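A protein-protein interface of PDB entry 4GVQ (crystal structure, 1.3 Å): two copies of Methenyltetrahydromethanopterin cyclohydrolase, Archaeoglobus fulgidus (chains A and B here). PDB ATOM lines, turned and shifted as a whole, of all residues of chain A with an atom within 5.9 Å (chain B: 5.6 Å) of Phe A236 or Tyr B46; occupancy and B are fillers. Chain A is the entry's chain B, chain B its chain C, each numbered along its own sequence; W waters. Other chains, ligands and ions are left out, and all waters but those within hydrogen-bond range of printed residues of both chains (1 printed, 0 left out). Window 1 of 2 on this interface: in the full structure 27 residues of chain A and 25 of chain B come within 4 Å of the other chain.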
ATOM      1  N   TYR A  81     -28.966   3.394  14.190  1.00  0.00           N
ATOM      2  CA  TYR A  81     -29.736   2.177  13.913  1.00  0.00           C
ATOM      3  C   TYR A  81     -30.439   1.685  15.161  1.00  0.00           C
ATOM      4  O   TYR A  81     -30.057   2.033  16.295  1.00  0.00           O
ATOM      5  CB  TYR A  81     -28.861   1.056  13.266  1.00  0.00           C
ATOM      6  CG  TYR A  81     -27.627   0.737  14.095  1.00  0.00           C
ATOM      7  CD1 TYR A  81     -26.386   1.337  13.833  1.00  0.00           C
ATOM      8  CD2 TYR A  81     -27.715  -0.174  15.167  1.00  0.00           C
ATOM      9  CE1 TYR A  81     -25.260   1.037  14.582  1.00  0.00           C
ATOM     10  CE2 TYR A  81     -26.609  -0.461  15.936  1.00  0.00           C
ATOM     11  CZ  TYR A  81     -25.393   0.145  15.663  1.00  0.00           C
ATOM     12  OH  TYR A  81     -24.291  -0.107  16.427  1.00  0.00           O
ATOM     13  N   THR A  82     -31.485   0.911  14.944  1.00  0.00           N
ATOM     14  CA  THR A  82     -32.235   0.342  16.056  1.00  0.00           C
ATOM     15  C   THR A  82     -32.847  -0.986  15.654  1.00  0.00           C
ATOM     16  O   THR A  82     -33.304  -1.161  14.530  1.00  0.00           O
ATOM     17  CB  THR A  82     -33.362   1.319  16.531  1.00  0.00           C
ATOM     18  OG1 THR A  82     -34.044   0.726  17.647  1.00  0.00           O
ATOM     19  CG2 THR A  82     -34.354   1.656  15.435  1.00  0.00           C
ATOM     20  N   ASP A  83     -32.905  -1.895  16.628  1.00  0.00           N
ATOM     21  CA  ASP A  83     -33.626  -3.144  16.473  1.00  0.00           C
ATOM     22  C   ASP A  83     -34.919  -3.180  17.272  1.00  0.00           C
ATOM     23  O   ASP A  83     -35.524  -4.262  17.451  1.00  0.00           O
ATOM     24  CB  ASP A  83     -32.682  -4.302  16.827  1.00  0.00           C
ATOM     25  CG  ASP A  83     -31.694  -4.555  15.718  1.00  0.00           C
ATOM     26  OD1 ASP A  83     -30.592  -3.923  15.744  1.00  0.00           O
ATOM     27  OD2 ASP A  83     -32.047  -5.313  14.780  1.00  0.00           O
ATOM     28  N   SER A 204     -36.138  -3.780  11.977  1.00  0.00           N
ATOM     29  CA  SER A 204     -35.026  -2.891  12.322  1.00  0.00           C
ATOM     30  C   SER A 204     -34.937  -1.778  11.330  1.00  0.00           C
ATOM     31  O   SER A 204     -35.545  -1.850  10.247  1.00  0.00           O
ATOM     32  CB  SER A 204     -33.712  -3.651  12.319  1.00  0.00           C
ATOM     33  OG  SER A 204     -33.517  -4.203  11.061  1.00  0.00           O
ATOM     34  N   GLY A 205     -34.149  -0.770  11.671  1.00  0.00           N
ATOM     35  CA  GLY A 205     -33.884   0.309  10.722  1.00  0.00           C
ATOM     36  C   GLY A 205     -32.555   0.951  10.994  1.00  0.00           C
ATOM     37  O   GLY A 205     -32.097   1.004  12.148  1.00  0.00           O
ATOM     38  N   ALA A 206     -31.932   1.457   9.933  1.00  0.00           N
ATOM     39  CA  ALA A 206     -30.639   2.112  10.001  1.00  0.00           C
ATOM     40  C   ALA A 206     -30.741   3.345   9.110  1.00  0.00           C
ATOM     41  O   ALA A 206     -31.284   3.273   8.027  1.00  0.00           O
ATOM     42  CB  ALA A 206     -29.519   1.156   9.532  1.00  0.00           C
ATOM     43  N   GLY A 207     -30.231   4.477   9.569  1.00  0.00           N
ATOM     44  CA  GLY A 207     -30.376   5.697   8.798  1.00  0.00           C
ATOM     45  C   GLY A 207     -29.169   6.598   8.849  1.00  0.00           C
ATOM     46  O   GLY A 207     -28.349   6.541   9.775  1.00  0.00           O
ATOM     47  N   SER A 234     -31.544   9.016   4.345  1.00  0.00           N
ATOM     48  CA  SER A 234     -31.563   7.686   3.760  1.00  0.00           C
ATOM     49  C   SER A 234     -31.781   6.627   4.844  1.00  0.00           C
ATOM     50  O   SER A 234     -31.132   6.690   5.886  1.00  0.00           O
ATOM     51  CB  SER A 234     -30.219   7.415   3.090  1.00  0.00           C
ATOM     52  OG  SER A 234     -29.913   8.372   2.109  1.00  0.00           O
ATOM     53  N   VAL A 235     -32.667   5.671   4.583  1.00  0.00           N
ATOM     54  CA  VAL A 235     -32.975   4.641   5.577  1.00  0.00           C
ATOM     55  C   VAL A 235     -32.950   3.259   4.921  1.00  0.00           C
ATOM     56  O   VAL A 235     -33.554   3.043   3.876  1.00  0.00           O
ATOM     57  CB  VAL A 235     -34.363   4.879   6.215  1.00  0.00           C
ATOM     58  CG1 VAL A 235     -34.612   3.840   7.292  1.00  0.00           C
ATOM     59  CG2 VAL A 235     -34.483   6.289   6.806  1.00  0.00           C
ATOM     60  N   PHE A 236     -32.213   2.339   5.546  1.00  0.00           N
ATOM     61  CA  PHE A 236     -32.281   0.913   5.236  1.00  0.00           C
ATOM     62  C   PHE A 236     -33.148   0.244   6.333  1.00  0.00           C
ATOM     63  O   PHE A 236     -32.815   0.309   7.510  1.00  0.00           O
ATOM     64  CB  PHE A 236     -30.879   0.300   5.188  1.00  0.00           C
ATOM     65  CG  PHE A 236     -30.877  -1.161   4.847  1.00  0.00           C
ATOM     66  CD1 PHE A 236     -30.662  -1.571   3.542  1.00  0.00           C
ATOM     67  CD2 PHE A 236     -31.047  -2.133   5.855  1.00  0.00           C
ATOM     68  CE1 PHE A 236     -30.681  -2.932   3.232  1.00  0.00           C
ATOM     69  CE2 PHE A 236     -31.065  -3.500   5.538  1.00  0.00           C
ATOM     70  CZ  PHE A 236     -30.863  -3.890   4.226  1.00  0.00           C
ATOM     71  N   LEU A 237     -34.264  -0.362   5.931  1.00  0.00           N
ATOM     72  CA  LEU A 237     -35.230  -0.987   6.841  1.00  0.00           C
ATOM     73  C   LEU A 237     -35.378  -2.456   6.566  1.00  0.00           C
ATOM     74  O   LEU A 237     -35.305  -2.860   5.398  1.00  0.00           O
ATOM     75  CB  LEU A 237     -36.631  -0.379   6.602  1.00  0.00           C
ATOM     76  CG  LEU A 237     -36.782   1.090   6.849  1.00  0.00           C
ATOM     77  CD1 LEU A 237     -37.723   1.733   5.876  1.00  0.00           C
ATOM     78  CD2 LEU A 237     -37.282   1.371   8.248  1.00  0.00           C
ATOM     79  N   THR A 238     -35.695  -3.225   7.593  1.00  0.00           N
ATOM     80  CA  THR A 238     -36.013  -4.621   7.432  1.00  0.00           C
ATOM     81  C   THR A 238     -37.413  -4.849   7.952  1.00  0.00           C
ATOM     82  O   THR A 238     -37.766  -4.379   9.055  1.00  0.00           O
ATOM     83  CB  THR A 238     -34.990  -5.421   8.212  1.00  0.00           C
ATOM     84  OG1 THR A 238     -33.688  -5.055   7.744  1.00  0.00           O
ATOM     85  CG2 THR A 238     -35.217  -6.934   8.017  1.00  0.00           C
ATOM     86  N   GLN A 284     -35.148   8.828   0.883  1.00  0.00           N
ATOM     87  CA  GLN A 284     -34.866   7.566   0.169  1.00  0.00           C
ATOM     88  C   GLN A 284     -34.865   6.397   1.145  1.00  0.00           C
ATOM     89  O   GLN A 284     -34.307   6.506   2.243  1.00  0.00           O
ATOM     90  CB  GLN A 284     -33.535   7.630  -0.617  1.00  0.00           C
ATOM     91  CG  GLN A 284     -33.335   6.475  -1.613  1.00  0.00           C
ATOM     92  CD  GLN A 284     -32.405   6.787  -2.774  1.00  0.00           C
ATOM     93  OE1 GLN A 284     -31.724   7.810  -2.782  1.00  0.00           O
ATOM     94  NE2 GLN A 284     -32.358   5.874  -3.761  1.00  0.00           N
ATOM     95  N   ILE A 285     -35.498   5.284   0.760  1.00  0.00           N
ATOM     96  CA  ILE A 285     -35.461   4.055   1.566  1.00  0.00           C
ATOM     97  C   ILE A 285     -35.097   2.822   0.758  1.00  0.00           C
ATOM     98  O   ILE A 285     -35.350   2.759  -0.443  1.00  0.00           O
ATOM     99  CB  ILE A 285     -36.800   3.774   2.268  1.00  0.00           C
ATOM    100  CG1 ILE A 285     -37.954   3.587   1.279  1.00  0.00           C
ATOM    101  CG2 ILE A 285     -37.134   4.895   3.223  1.00  0.00           C
ATOM    102  CD1 ILE A 285     -39.248   3.159   1.938  1.00  0.00           C
ATOM    103  N   ALA A 286     -34.489   1.844   1.432  1.00  0.00           N
ATOM    104  CA  ALA A 286     -34.318   0.489   0.921  1.00  0.00           C
ATOM    105  C   ALA A 286     -35.029  -0.397   1.940  1.00  0.00           C
ATOM    106  O   ALA A 286     -34.771  -0.284   3.144  1.00  0.00           O
ATOM    107  CB  ALA A 286     -32.858   0.112   0.791  1.00  0.00           C
ATOM    108  N   VAL A 287     -35.911  -1.279   1.488  1.00  0.00           N
ATOM    109  CA  VAL A 287     -36.744  -2.101   2.385  1.00  0.00           C
ATOM    110  C   VAL A 287     -36.471  -3.585   2.106  1.00  0.00           C
ATOM    111  O   VAL A 287     -36.859  -4.109   1.045  1.00  0.00           O
ATOM    112  CB  VAL A 287     -38.241  -1.820   2.186  1.00  0.00           C
ATOM    113  CG1 VAL A 287     -39.084  -2.667   3.148  1.00  0.00           C
ATOM    114  CG2 VAL A 287     -38.559  -0.331   2.344  1.00  0.00           C
ATOM    115  N   ASN A 288     -35.751  -4.241   3.016  1.00  0.00           N
ATOM    116  CA  ASN A 288     -35.438  -5.656   2.917  1.00  0.00           C
ATOM    117  C   ASN A 288     -36.629  -6.437   3.472  1.00  0.00           C
ATOM    118  O   ASN A 288     -36.951  -6.355   4.657  1.00  0.00           O
ATOM    119  CB  ASN A 288     -34.166  -5.923   3.702  1.00  0.00           C
ATOM    120  CG  ASN A 288     -33.812  -7.401   3.828  1.00  0.00           C
ATOM    121  OD1 ASN A 288     -34.180  -8.260   2.988  1.00  0.00           O
ATOM    122  ND2 ASN A 288     -33.025  -7.697   4.825  1.00  0.00           N
ATOM    123  N   THR A 295     -35.069  -6.704  -1.733  1.00  0.00           N
ATOM    124  CA  THR A 295     -34.890  -5.392  -1.114  1.00  0.00           C
ATOM    125  C   THR A 295     -35.344  -4.339  -2.112  1.00  0.00           C
ATOM    126  O   THR A 295     -34.758  -4.190  -3.187  1.00  0.00           O
ATOM    127  CB  THR A 295     -33.462  -5.135  -0.629  1.00  0.00           C
ATOM    128  OG1 THR A 295     -33.186  -6.019   0.472  1.00  0.00           O
ATOM    129  CG2 THR A 295     -33.292  -3.691  -0.144  1.00  0.00           C
ATOM    130  N   GLY B  44     -31.888 -11.420  17.092  1.00  0.00           N
ATOM    131  CA  GLY B  44     -30.606 -10.742  17.194  1.00  0.00           C
ATOM    132  C   GLY B  44     -30.778  -9.266  16.797  1.00  0.00           C
ATOM    133  O   GLY B  44     -31.887  -8.726  16.779  1.00  0.00           O
ATOM    134  N   SER B  45     -29.653  -8.610  16.562  1.00  0.00           N
ATOM    135  CA  SER B  45     -29.637  -7.151  16.363  1.00  0.00           C
ATOM    136  C   SER B  45     -28.326  -6.765  15.740  1.00  0.00           C
ATOM    137  O   SER B  45     -27.353  -7.523  15.742  1.00  0.00           O
ATOM    138  CB  SER B  45     -29.769  -6.440  17.733  1.00  0.00           C
ATOM    139  OG  SER B  45     -28.747  -6.835  18.621  1.00  0.00           O
ATOM    140  N   TYR B  46     -28.288  -5.538  15.225  1.00  0.00           N
ATOM    141  CA  TYR B  46     -27.033  -4.965  14.763  1.00  0.00           C
ATOM    142  C   TYR B  46     -25.945  -5.011  15.825  1.00  0.00           C
ATOM    143  O   TYR B  46     -24.821  -5.422  15.550  1.00  0.00           O
ATOM    144  CB  TYR B  46     -27.233  -3.543  14.285  1.00  0.00           C
ATOM    145  CG  TYR B  46     -27.912  -3.393  12.956  1.00  0.00           C
ATOM    146  CD1 TYR B  46     -29.149  -2.767  12.836  1.00  0.00           C
ATOM    147  CD2 TYR B  46     -27.272  -3.825  11.781  1.00  0.00           C
ATOM    148  CE1 TYR B  46     -29.747  -2.569  11.582  1.00  0.00           C
ATOM    149  CE2 TYR B  46     -27.857  -3.637  10.536  1.00  0.00           C
ATOM    150  CZ  TYR B  46     -29.092  -2.991  10.445  1.00  0.00           C
ATOM    151  OH  TYR B  46     -29.691  -2.796   9.230  1.00  0.00           O
ATOM    152  N   ASP B  47     -26.271  -4.593  17.058  1.00  0.00           N
ATOM    153  CA  ASP B  47     -25.274  -4.612  18.111  1.00  0.00           C
ATOM    154  C   ASP B  47     -24.847  -6.023  18.473  1.00  0.00           C
ATOM    155  O   ASP B  47     -23.670  -6.239  18.732  1.00  0.00           O
ATOM    156  CB  ASP B  47     -25.739  -3.846  19.362  1.00  0.00           C
ATOM    157  CG  ASP B  47     -25.560  -2.364  19.249  1.00  0.00           C
ATOM    158  OD1 ASP B  47     -24.790  -1.882  18.396  1.00  0.00           O
ATOM    159  OD2 ASP B  47     -26.181  -1.669  20.067  1.00  0.00           O
ATOM    160  N   ALA B  48     -25.795  -6.982  18.485  1.00  0.00           N
ATOM    161  CA  ALA B  48     -25.355  -8.356  18.730  1.00  0.00           C
ATOM    162  C   ALA B  48     -24.419  -8.813  17.606  1.00  0.00           C
ATOM    163  O   ALA B  48     -23.448  -9.530  17.874  1.00  0.00           O
ATOM    164  CB  ALA B  48     -26.513  -9.325  18.845  1.00  0.00           C
ATOM    165  N   GLY B  49     -24.641  -8.349  16.366  1.00  0.00           N
ATOM    166  CA  GLY B  49     -23.745  -8.691  15.271  1.00  0.00           C
ATOM    167  C   GLY B  49     -22.369  -8.103  15.451  1.00  0.00           C
ATOM    168  O   GLY B  49     -21.346  -8.757  15.193  1.00  0.00           O
ATOM    169  N   ILE B  50     -22.318  -6.841  15.885  1.00  0.00           N
ATOM    170  CA  ILE B  50     -21.028  -6.222  16.177  1.00  0.00           C
ATOM    171  C   ILE B  50     -20.276  -6.998  17.252  1.00  0.00           C
ATOM    172  O   ILE B  50     -19.071  -7.301  17.114  1.00  0.00           O
ATOM    173  CB  ILE B  50     -21.200  -4.751  16.621  1.00  0.00           C
ATOM    174  CG1 ILE B  50     -21.625  -3.884  15.427  1.00  0.00           C
ATOM    175  CG2 ILE B  50     -19.908  -4.239  17.231  1.00  0.00           C
ATOM    176  CD1 ILE B  50     -22.053  -2.486  15.821  1.00  0.00           C
ATOM    177  N   MET B  51     -20.979  -7.336  18.334  1.00  0.00           N
ATOM    178  CA  MET B  51     -20.318  -8.023  19.463  1.00  0.00           C
ATOM    179  C   MET B  51     -19.902  -9.447  19.059  1.00  0.00           C
ATOM    180  O   MET B  51     -18.796  -9.888  19.426  1.00  0.00           O
ATOM    181  CB  MET B  51     -21.228  -8.054  20.681  1.00  0.00           C
ATOM    182  CG  MET B  51     -21.483  -6.628  21.144  1.00  0.00           C
ATOM    183  SD  MET B  51     -22.634  -6.471  22.516  1.00  0.00           S
ATOM    184  CE  MET B  51     -21.492  -6.666  23.885  1.00  0.00           C
ATOM    185  N   ILE B  65     -20.558   0.002  12.880  1.00  0.00           N
ATOM    186  CA  ILE B  65     -21.448   0.072  11.742  1.00  0.00           C
ATOM    187  C   ILE B  65     -21.709   1.546  11.424  1.00  0.00           C
ATOM    188  O   ILE B  65     -21.977   2.353  12.325  1.00  0.00           O
ATOM    189  CB  ILE B  65     -22.779  -0.649  12.036  1.00  0.00           C
ATOM    190  CG1 ILE B  65     -22.483  -2.168  12.092  1.00  0.00           C
ATOM    191  CG2 ILE B  65     -23.868  -0.268  11.001  1.00  0.00           C
ATOM    192  CD1 ILE B  65     -23.698  -2.988  12.496  1.00  0.00           C
ATOM    193  N   VAL B  67     -23.854   3.913   8.300  1.00  0.00           N
ATOM    194  CA  VAL B  67     -24.809   3.830   7.190  1.00  0.00           C
ATOM    195  C   VAL B  67     -24.280   4.735   6.072  1.00  0.00           C
ATOM    196  O   VAL B  67     -23.868   5.870   6.334  1.00  0.00           O
ATOM    197  CB  VAL B  67     -26.218   4.271   7.640  1.00  0.00           C
ATOM    198  CG1 VAL B  67     -27.213   4.220   6.488  1.00  0.00           C
ATOM    199  CG2 VAL B  67     -26.691   3.379   8.781  1.00  0.00           C
ATOM    200  N   PRO B  74     -29.187   3.165   0.180  1.00  0.00           N
ATOM    201  CA  PRO B  74     -28.611   3.081   1.545  1.00  0.00           C
ATOM    202  C   PRO B  74     -28.363   1.661   1.988  1.00  0.00           C
ATOM    203  O   PRO B  74     -29.213   0.792   1.738  1.00  0.00           O
ATOM    204  CB  PRO B  74     -29.663   3.724   2.443  1.00  0.00           C
ATOM    205  CG  PRO B  74     -30.912   3.728   1.653  1.00  0.00           C
ATOM    206  CD  PRO B  74     -30.606   3.589   0.182  1.00  0.00           C
ATOM    207  N   PHE B  75     -27.224   1.446   2.624  1.00  0.00           N
ATOM    208  CA  PHE B  75     -26.888   0.166   3.262  1.00  0.00           C
ATOM    209  C   PHE B  75     -26.214   0.459   4.580  1.00  0.00           C
ATOM    210  O   PHE B  75     -25.555   1.488   4.745  1.00  0.00           O
ATOM    211  CB  PHE B  75     -25.919  -0.670   2.404  1.00  0.00           C
ATOM    212  CG  PHE B  75     -26.536  -1.139   1.118  1.00  0.00           C
ATOM    213  CD1 PHE B  75     -26.362  -0.422  -0.066  1.00  0.00           C
ATOM    214  CD2 PHE B  75     -27.382  -2.257   1.097  1.00  0.00           C
ATOM    215  CE1 PHE B  75     -26.957  -0.853  -1.239  1.00  0.00           C
ATOM    216  CE2 PHE B  75     -27.957  -2.715  -0.085  1.00  0.00           C
ATOM    217  CZ  PHE B  75     -27.760  -2.004  -1.246  1.00  0.00           C
ATOM    218  N   ALA B  76     -26.324  -0.473   5.523  1.00  0.00           N
ATOM    219  CA  ALA B  76     -25.433  -0.447   6.678  1.00  0.00           C
ATOM    220  C   ALA B  76     -24.093  -1.069   6.235  1.00  0.00           C
ATOM    221  O   ALA B  76     -24.085  -2.040   5.449  1.00  0.00           O
ATOM    222  CB  ALA B  76     -26.028  -1.216   7.846  1.00  0.00           C
ATOM    223  N   ILE B 174     -29.608 -11.254  10.920  1.00  0.00           N
ATOM    224  CA  ILE B 174     -28.839 -10.005  10.958  1.00  0.00           C
ATOM    225  C   ILE B 174     -27.454 -10.227  11.550  1.00  0.00           C
ATOM    226  O   ILE B 174     -26.455  -9.707  11.038  1.00  0.00           O
ATOM    227  CB  ILE B 174     -29.561  -8.821  11.620  1.00  0.00           C
ATOM    228  CG1 ILE B 174     -28.777  -7.532  11.350  1.00  0.00           C
ATOM    229  CG2 ILE B 174     -29.769  -9.041  13.105  1.00  0.00           C
ATOM    230  CD1 ILE B 174     -28.636  -7.145   9.865  1.00  0.00           C
ATOM    231  N   VAL B 178     -23.995  -9.346   9.564  1.00  0.00           N
ATOM    232  CA  VAL B 178     -22.963  -8.462  10.127  1.00  0.00           C
ATOM    233  C   VAL B 178     -21.647  -9.203  10.308  1.00  0.00           C
ATOM    234  O   VAL B 178     -20.605  -8.685   9.978  1.00  0.00           O
ATOM    235  CB  VAL B 178     -23.424  -7.863  11.476  1.00  0.00           C
ATOM    236  CG1 VAL B 178     -22.285  -7.085  12.150  1.00  0.00           C
ATOM    237  CG2 VAL B 178     -24.633  -6.945  11.247  1.00  0.00           C
ATOM    238  N   ILE B 211     -23.208  -4.569   4.622  1.00  0.00           N
ATOM    239  CA  ILE B 211     -23.884  -5.666   5.290  1.00  0.00           C
ATOM    240  C   ILE B 211     -25.031  -6.146   4.424  1.00  0.00           C
ATOM    241  O   ILE B 211     -25.928  -5.383   4.049  1.00  0.00           O
ATOM    242  CB  ILE B 211     -24.379  -5.187   6.665  1.00  0.00           C
ATOM    243  CG1 ILE B 211     -23.195  -4.837   7.575  1.00  0.00           C
ATOM    244  CG2 ILE B 211     -25.297  -6.216   7.308  1.00  0.00           C
ATOM    245  CD1 ILE B 211     -23.556  -3.930   8.725  1.00  0.00           C
ATOM    246  N   SER B 212     -25.032  -7.427   4.081  1.00  0.00           N
ATOM    247  CA  SER B 212     -26.054  -7.942   3.158  1.00  0.00           C
ATOM    248  C   SER B 212     -27.451  -7.838   3.742  1.00  0.00           C
ATOM    249  O   SER B 212     -27.655  -8.148   4.918  1.00  0.00           O
ATOM    250  CB  SER B 212     -25.790  -9.430   2.870  1.00  0.00           C
ATOM    251  OG  SER B 212     -26.747  -9.964   1.972  1.00  0.00           O
ATOM    252  N   PRO B 213     -28.444  -7.478   2.926  1.00  0.00           N
ATOM    253  CA  PRO B 213     -29.820  -7.766   3.300  1.00  0.00           C
ATOM    254  C   PRO B 213     -29.960  -9.250   3.636  1.00  0.00           C
ATOM    255  O   PRO B 213     -29.160 -10.075   3.207  1.00  0.00           O
ATOM    256  CB  PRO B 213     -30.613  -7.438   2.027  1.00  0.00           C
ATOM    257  CG  PRO B 213     -29.706  -6.545   1.244  1.00  0.00           C
ATOM    258  CD  PRO B 213     -28.301  -6.962   1.552  1.00  0.00           C
HETATM  259  O   HOH W   1     -32.519  -2.687   8.998  1.00  0.00           O
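O of Ala A206 is in hydrogen-bond range of N of Phe A236 (2.8 Å).
The backbone NH of Val A235 lies within hydrogen-bond range of the backbone carbonyl oxygen of Gln A284.
O of Val A235 sits at hydrogen-bond distance from N of Ala A286 (2.9 Å).
N of Leu A237 lies within hydrogen-bond range of O of Ala A286 (2.8 Å).
The backbone NH of Asn A288 is in hydrogen-bond range of the backbone carbonyl oxygen of Leu A237 (2.8 Å).
The backbone NH (N) of Ala B48 lies within hydrogen-bond range of the side-chain hydroxyl (OG) of Ser B45 (3.0 Å).
Printed residues of chain A that touch a printed residue of chain B: Tyr A81, Asp A83, Ala A206, Gly A207, Ser A234, Val A235, Phe A236, Ala A286, Asn A288 and Thr A295.
Hydrophobic or aromatic side chains of chain A within 4 Å of the printed part of chain B: Tyr A81, Ala A206, Phe A236 and Ala A286.
Among the printed residues, 18 pairs touch across the chains.
Water W1 lies within hydrogen-bond range of the side-chain hydroxyl (OG) of Ser A204 (2.7 Å), the side-chain hydroxyl (OH) of Tyr B46 (2.8 Å), the side-chain hydroxyl (OG1) of Thr A238 (2.9 Å) and the backbone carbonyl oxygen (O) of Phe A236 (3.4 Å).
Of the printed residues of chain B, Phe A236 touches Tyr B46 (3.7 Å), Pro B74 (3.3 Å) and Phe B75 (3.99 Å).
Printed residues of chain A within 4 Å of Tyr B46: Tyr A81, Asp A83, Ala A206 and Phe A236.
Printed residues of chain B within 4 Å of Ser A234: Pro B74.
Printed residues of chain A within 4 Å of Ile B65: Tyr A81.
Printed residues of chain A within 4 Å of Ile B50: Tyr A81.
The nearest residue of chain A that does not touch Tyr B46 is Ser A204 (4.1 Å).
The nearest printed residue of chain B that does not touch Asn A288 is Ser B212 (5.4 Å).
The side-chain carboxylate (OD1) of Asp B47 lies within hydrogen-bond range of the side-chain hydroxyl (OH) of Tyr A81 (2.7 Å).
OD1 of Asp A83 is in hydrogen-bond range of N of Tyr B46.
No position is printed for both chains.
Among the printed residues, merely in contact across the chains: Phe A236 with Pro B74 (3.3 Å), Asp A83 with Ser B45 (3.3 Å), Tyr A81 with Ile B50 (3.3 Å), Thr A295 with Pro B213 (3.3 Å), Tyr A81 with Tyr B46 (3.5 Å), Val A235 with Pro B74 (3.5 Å), Asn A288 with Pro B213 (3.5 Å), Ala A206 with Val B67 (3.7 Å), Phe A236 with Tyr B46 (3.7 Å), Gly A207 with Val B67 (3.7 Å), Ser A234 with Pro B74 (3.8 Å), Ala A286 with Pro B74 (3.8 Å), Tyr A81 with Ile B65 (3.9 Å), Asp A83 with Gly B44 (3.96 Å), Ala A206 with Tyr B46 (3.97 Å) and Phe A236 with Phe B75 (3.99 Å).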
